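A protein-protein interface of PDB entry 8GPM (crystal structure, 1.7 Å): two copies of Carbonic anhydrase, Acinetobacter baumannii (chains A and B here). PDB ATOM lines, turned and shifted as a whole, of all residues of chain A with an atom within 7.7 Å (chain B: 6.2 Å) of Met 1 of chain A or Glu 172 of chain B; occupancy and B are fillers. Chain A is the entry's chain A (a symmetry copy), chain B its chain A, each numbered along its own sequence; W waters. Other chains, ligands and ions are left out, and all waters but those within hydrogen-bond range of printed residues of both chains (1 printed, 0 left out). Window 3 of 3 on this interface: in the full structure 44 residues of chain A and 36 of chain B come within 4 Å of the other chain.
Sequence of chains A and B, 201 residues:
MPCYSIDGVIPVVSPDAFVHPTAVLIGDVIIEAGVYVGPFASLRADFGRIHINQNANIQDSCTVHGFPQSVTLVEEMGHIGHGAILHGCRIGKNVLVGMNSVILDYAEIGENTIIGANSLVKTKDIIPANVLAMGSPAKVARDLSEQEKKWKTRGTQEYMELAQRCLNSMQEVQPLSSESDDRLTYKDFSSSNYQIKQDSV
Hydrophobic or aromatic side chains of chain B that line the printed part of chain A: Pro 21, Met 170 and Val 173. Hydrophobic or aromatic side chains of chain A that line the printed part of chain B: Met 1 and Tyr 4. Along chain A the printed residues that touch a printed residue of chain B span positions 1 to 5. Among the printed residues, 11 pairs touch across the chains. Among the printed residues, no Asp or Glu carboxylate lies within 4 Å of a Lys or Arg side-chain nitrogen of the other chain.
O of Gln 171 of chain B is in hydrogen-bond range of N of Ser 5 of chain A (2.9 Å). The backbone NH (N) of Val 173 of chain B lies within hydrogen-bond range of the backbone carbonyl oxygen (O) of Cys 3 of chain A.
Water W1 lies within hydrogen-bond range of OH of Tyr 4 of chain A and OE2 of Glu 172 of chain B.
Position printed for both chains: 21.
The backbone NH (N) of Tyr 4 of chain A lies within hydrogen-bond range of the backbone carbonyl oxygen (O) of Leu 25 of chain A.
Met 1 of chain A touches one residue of chain B. Glu 172 of chain B touches just these residues of chain A: Met 1, Cys 3 and Tyr 4. Printed residues of chain B within 4 Å of Tyr 4 of chain A: Pro 21, Met 170, Gln 171, Glu 172 and Val 173. Of the printed residues of chain A, Met 170 of chain B touches Tyr 4 and Ser 5. Of the printed residues of chain B, Ser 5 of chain A touches Met 170, Gln 171 and Val 173. Printed residues of chain A within 4 Å of Pro 21 of chain B: Tyr 4 (3.9 Å). Printed residues of chain B within 4 Å of Cys 3 of chain A: Glu 172 (3.4 Å) and Val 173 (3.0 Å). The nearest residue of chain A that does not touch Glu 172 of chain B is Ser 5 of chain A (5.1 Å). The nearest printed residue of chain A that does not touch Pro 21 of chain B is Val 24 of chain A (7.0 Å).
Among the printed residues, pairs that only touch across the chains: Met 1 of chain A with Glu 172 of chain B, Cys 3 of chain A with Glu 172 of chain B, Tyr 4 of chain A with Pro 21 of chain B, Tyr 4 of chain A with Met 170 of chain B, Tyr 4 of chain A with Gln 171 of chain B, Tyr 4 of chain A with Glu 172 of chain B, Tyr 4 of chain A with Val 173 of chain B, Ser 5 of chain A with Met 170 of chain B and Ser 5 of chain A with Val 173 of chain B.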
ATOM      1  N   MET A   1      -4.901   9.228 -10.235  1.00  0.00           N
ATOM      2  CA  MET A   1      -6.304   8.983 -10.589  1.00  0.00           C
ATOM      3  C   MET A   1      -6.447   8.724 -12.093  1.00  0.00           C
ATOM      4  O   MET A   1      -6.186   9.621 -12.903  1.00  0.00           O
ATOM      5  CB  MET A   1      -7.182  10.181 -10.173  1.00  0.00           C
ATOM      6  N   PRO A   2      -6.855   7.516 -12.502  1.00  0.00           N
ATOM      7  CA  PRO A   2      -6.927   7.267 -13.940  1.00  0.00           C
ATOM      8  C   PRO A   2      -8.170   7.852 -14.586  1.00  0.00           C
ATOM      9  O   PRO A   2      -8.193   7.902 -15.812  1.00  0.00           O
ATOM     10  CB  PRO A   2      -6.895   5.718 -14.054  1.00  0.00           C
ATOM     11  CG  PRO A   2      -7.378   5.201 -12.749  1.00  0.00           C
ATOM     12  CD  PRO A   2      -7.340   6.358 -11.721  1.00  0.00           C
ATOM     13  N   CYS A   3      -9.155   8.362 -13.824  1.00  0.00           N
ATOM     14  CA  CYS A   3     -10.431   8.797 -14.406  1.00  0.00           C
ATOM     15  C   CYS A   3     -10.524  10.317 -14.549  1.00  0.00           C
ATOM     16  O   CYS A   3     -10.109  11.074 -13.664  1.00  0.00           O
ATOM     17  CB  CYS A   3     -11.614   8.276 -13.574  1.00  0.00           C
ATOM     18  SG  CYS A   3     -11.728   6.451 -13.633  1.00  0.00           S
ATOM     19  N   TYR A   4     -11.048  10.764 -15.697  1.00  0.00           N
ATOM     20  CA  TYR A   4     -11.193  12.183 -16.013  1.00  0.00           C
ATOM     21  C   TYR A   4     -12.586  12.404 -16.541  1.00  0.00           C
ATOM     22  O   TYR A   4     -13.055  11.601 -17.350  1.00  0.00           O
ATOM     23  CB  TYR A   4     -10.219  12.663 -17.122  1.00  0.00           C
ATOM     24  CG  TYR A   4      -8.784  12.640 -16.711  1.00  0.00           C
ATOM     25  CD1 TYR A   4      -8.059  11.439 -16.696  1.00  0.00           C
ATOM     26  CD2 TYR A   4      -8.150  13.814 -16.339  1.00  0.00           C
ATOM     27  CE1 TYR A   4      -6.734  11.404 -16.293  1.00  0.00           C
ATOM     28  CE2 TYR A   4      -6.807  13.790 -15.943  1.00  0.00           C
ATOM     29  CZ  TYR A   4      -6.116  12.593 -15.930  1.00  0.00           C
ATOM     30  OH  TYR A   4      -4.789  12.554 -15.517  1.00  0.00           O
ATOM     31  N   SER A   5     -13.257  13.468 -16.084  1.00  0.00           N
ATOM     32  CA  SER A   5     -14.529  13.829 -16.686  1.00  0.00           C
ATOM     33  C   SER A   5     -14.306  14.834 -17.814  1.00  0.00           C
ATOM     34  O   SER A   5     -13.261  15.481 -17.919  1.00  0.00           O
ATOM     35  CB  SER A   5     -15.505  14.414 -15.652  1.00  0.00           C
ATOM     36  OG  SER A   5     -15.042  15.644 -15.109  1.00  0.00           O
ATOM     37  N   VAL A  19      -8.324  -1.345 -12.741  1.00  0.00           N
ATOM     38  CA  VAL A  19      -7.809  -0.375 -13.710  1.00  0.00           C
ATOM     39  C   VAL A  19      -6.441   0.051 -13.226  1.00  0.00           C
ATOM     40  O   VAL A  19      -6.323   0.620 -12.132  1.00  0.00           O
ATOM     41  CB  VAL A  19      -8.734   0.850 -13.852  1.00  0.00           C
ATOM     42  CG1 VAL A  19      -8.110   1.903 -14.804  1.00  0.00           C
ATOM     43  CG2 VAL A  19     -10.124   0.417 -14.345  1.00  0.00           C
ATOM     44  N   HIS A  20      -5.405  -0.215 -14.033  1.00  0.00           N
ATOM     45  CA  HIS A  20      -4.074   0.127 -13.581  1.00  0.00           C
ATOM     46  C   HIS A  20      -4.009   1.636 -13.348  1.00  0.00           C
ATOM     47  O   HIS A  20      -4.609   2.397 -14.101  1.00  0.00           O
ATOM     48  CB  HIS A  20      -2.995  -0.299 -14.585  1.00  0.00           C
ATOM     49  CG  HIS A  20      -1.623  -0.245 -13.983  1.00  0.00           C
ATOM     50  ND1 HIS A  20      -0.838   0.885 -14.053  1.00  0.00           N
ATOM     51  CD2 HIS A  20      -0.938  -1.139 -13.231  1.00  0.00           C
ATOM     52  CE1 HIS A  20       0.274   0.689 -13.361  1.00  0.00           C
ATOM     53  NE2 HIS A  20       0.245  -0.535 -12.865  1.00  0.00           N
ATOM     54  N   PRO A  21      -3.326   2.099 -12.299  1.00  0.00           N
ATOM     55  CA  PRO A  21      -3.283   3.543 -12.021  1.00  0.00           C
ATOM     56  C   PRO A  21      -2.732   4.375 -13.142  1.00  0.00           C
ATOM     57  O   PRO A  21      -2.996   5.585 -13.158  1.00  0.00           O
ATOM     58  CB  PRO A  21      -2.381   3.659 -10.781  1.00  0.00           C
ATOM     59  CG  PRO A  21      -2.170   2.301 -10.272  1.00  0.00           C
ATOM     60  CD  PRO A  21      -2.798   1.276 -11.193  1.00  0.00           C
ATOM     61  N   THR A  22      -1.971   3.788 -14.080  1.00  0.00           N
ATOM     62  CA  THR A  22      -1.443   4.551 -15.213  1.00  0.00           C
ATOM     63  C   THR A  22      -2.332   4.519 -16.455  1.00  0.00           C
ATOM     64  O   THR A  22      -1.986   5.172 -17.444  1.00  0.00           O
ATOM     65  CB  THR A  22      -0.030   4.066 -15.603  1.00  0.00           C
ATOM     66  OG1 THR A  22      -0.074   2.702 -16.080  1.00  0.00           O
ATOM     67  CG2 THR A  22       0.926   4.178 -14.412  1.00  0.00           C
ATOM     68  N   ALA A  23      -3.450   3.786 -16.446  1.00  0.00           N
ATOM     69  CA  ALA A  23      -4.358   3.921 -17.576  1.00  0.00           C
ATOM     70  C   ALA A  23      -5.096   5.258 -17.471  1.00  0.00           C
ATOM     71  O   ALA A  23      -4.982   5.981 -16.485  1.00  0.00           O
ATOM     72  CB  ALA A  23      -5.353   2.762 -17.620  1.00  0.00           C
ATOM     73  N   VAL A  24      -5.812   5.619 -18.538  1.00  0.00           N
ATOM     74  CA  VAL A  24      -6.608   6.850 -18.566  1.00  0.00           C
ATOM     75  C   VAL A  24      -7.994   6.491 -19.059  1.00  0.00           C
ATOM     76  O   VAL A  24      -8.128   5.948 -20.170  1.00  0.00           O
ATOM     77  CB  VAL A  24      -5.993   7.914 -19.496  1.00  0.00           C
ATOM     78  CG1 VAL A  24      -7.054   8.984 -19.877  1.00  0.00           C
ATOM     79  CG2 VAL A  24      -4.785   8.548 -18.841  1.00  0.00           C
ATOM     80  N   LEU A  25      -9.025   6.848 -18.262  1.00  0.00           N
ATOM     81  CA  LEU A  25     -10.418   6.706 -18.650  1.00  0.00           C
ATOM     82  C   LEU A  25     -10.984   8.110 -18.716  1.00  0.00           C
ATOM     83  O   LEU A  25     -10.866   8.862 -17.744  1.00  0.00           O
ATOM     84  CB  LEU A  25     -11.226   5.867 -17.634  1.00  0.00           C
ATOM     85  CG  LEU A  25     -11.173   4.338 -17.754  1.00  0.00           C
ATOM     86  CD1 LEU A  25      -9.818   3.778 -17.883  1.00  0.00           C
ATOM     87  CD2 LEU A  25     -11.854   3.780 -16.508  1.00  0.00           C
ATOM     88  N   PRO B  21      -2.641  15.726 -19.098  1.00  0.00           N
ATOM     89  CA  PRO B  21      -1.662  15.568 -18.011  1.00  0.00           C
ATOM     90  C   PRO B  21      -0.852  14.307 -18.085  1.00  0.00           C
ATOM     91  O   PRO B  21       0.218  14.260 -17.461  1.00  0.00           O
ATOM     92  CB  PRO B  21      -2.517  15.575 -16.733  1.00  0.00           C
ATOM     93  CG  PRO B  21      -3.870  15.985 -17.120  1.00  0.00           C
ATOM     94  CD  PRO B  21      -3.979  16.135 -18.623  1.00  0.00           C
ATOM     95  N   MET B 170     -11.963  19.447 -18.548  1.00  0.00           N
ATOM     96  CA  MET B 170     -11.493  18.120 -18.204  1.00  0.00           C
ATOM     97  C   MET B 170     -10.865  18.187 -16.811  1.00  0.00           C
ATOM     98  O   MET B 170     -10.107  19.120 -16.493  1.00  0.00           O
ATOM     99  CB  MET B 170     -10.543  17.568 -19.264  1.00  0.00           C
ATOM    100  CG  MET B 170      -9.627  16.431 -18.749  1.00  0.00           C
ATOM    101  SD  MET B 170      -9.081  15.479 -20.162  1.00  0.00           S
ATOM    102  CE  MET B 170     -10.594  15.073 -21.026  1.00  0.00           C
ATOM    103  N   GLN B 171     -11.262  17.259 -15.937  1.00  0.00           N
ATOM    104  CA  GLN B 171     -10.674  17.229 -14.603  1.00  0.00           C
ATOM    105  C   GLN B 171     -10.609  15.804 -14.084  1.00  0.00           C
ATOM    106  O   GLN B 171     -11.433  14.952 -14.432  1.00  0.00           O
ATOM    107  CB  GLN B 171     -11.450  18.116 -13.637  1.00  0.00           C
ATOM    108  CG  GLN B 171     -12.941  18.014 -13.788  1.00  0.00           C
ATOM    109  CD  GLN B 171     -13.677  19.067 -12.976  1.00  0.00           C
ATOM    110  OE1 GLN B 171     -13.974  18.864 -11.798  1.00  0.00           O
ATOM    111  NE2 GLN B 171     -13.990  20.199 -13.614  1.00  0.00           N
ATOM    112  N   GLU B 172      -9.609  15.555 -13.244  1.00  0.00           N
ATOM    113  CA  GLU B 172      -9.543  14.285 -12.538  1.00  0.00           C
ATOM    114  C   GLU B 172     -10.786  14.102 -11.667  1.00  0.00           C
ATOM    115  O   GLU B 172     -11.267  15.048 -11.043  1.00  0.00           O
ATOM    116  CB  GLU B 172      -8.294  14.243 -11.661  1.00  0.00           C
ATOM    117  CG  GLU B 172      -7.034  13.924 -12.407  1.00  0.00           C
ATOM    118  CD  GLU B 172      -5.843  13.781 -11.460  1.00  0.00           C
ATOM    119  OE1 GLU B 172      -5.779  14.544 -10.476  1.00  0.00           O
ATOM    120  OE2 GLU B 172      -4.982  12.908 -11.702  1.00  0.00           O
ATOM    121  N   VAL B 173     -11.304  12.870 -11.620  1.00  0.00           N
ATOM    122  CA  VAL B 173     -12.497  12.554 -10.845  1.00  0.00           C
ATOM    123  C   VAL B 173     -12.393  11.138 -10.299  1.00  0.00           C
ATOM    124  O   VAL B 173     -11.723  10.271 -10.869  1.00  0.00           O
ATOM    125  CB  VAL B 173     -13.796  12.720 -11.670  1.00  0.00           C
ATOM    126  CG1 VAL B 173     -13.839  14.084 -12.268  1.00  0.00           C
ATOM    127  CG2 VAL B 173     -13.808  11.677 -12.841  1.00  0.00           C
ATOM    128  N   GLN B 174     -13.072  10.918  -9.181  1.00  0.00           N
ATOM    129  CA  GLN B 174     -13.366   9.560  -8.753  1.00  0.00           C
ATOM    130  C   GLN B 174     -14.459   9.004  -9.667  1.00  0.00           C
ATOM    131  O   GLN B 174     -15.493   9.663  -9.861  1.00  0.00           O
ATOM    132  CB  GLN B 174     -13.845   9.531  -7.278  1.00  0.00           C
ATOM    133  CG  GLN B 174     -12.692   9.523  -6.256  1.00  0.00           C
ATOM    134  CD  GLN B 174     -11.855   8.248  -6.314  1.00  0.00           C
ATOM    135  OE1 GLN B 174     -12.300   7.178  -5.898  1.00  0.00           O
ATOM    136  NE2 GLN B 174     -10.633   8.366  -6.825  1.00  0.00           N
HETATM  137  O   HOH W   1      -3.920  14.508 -13.819  1.00  0.00           O
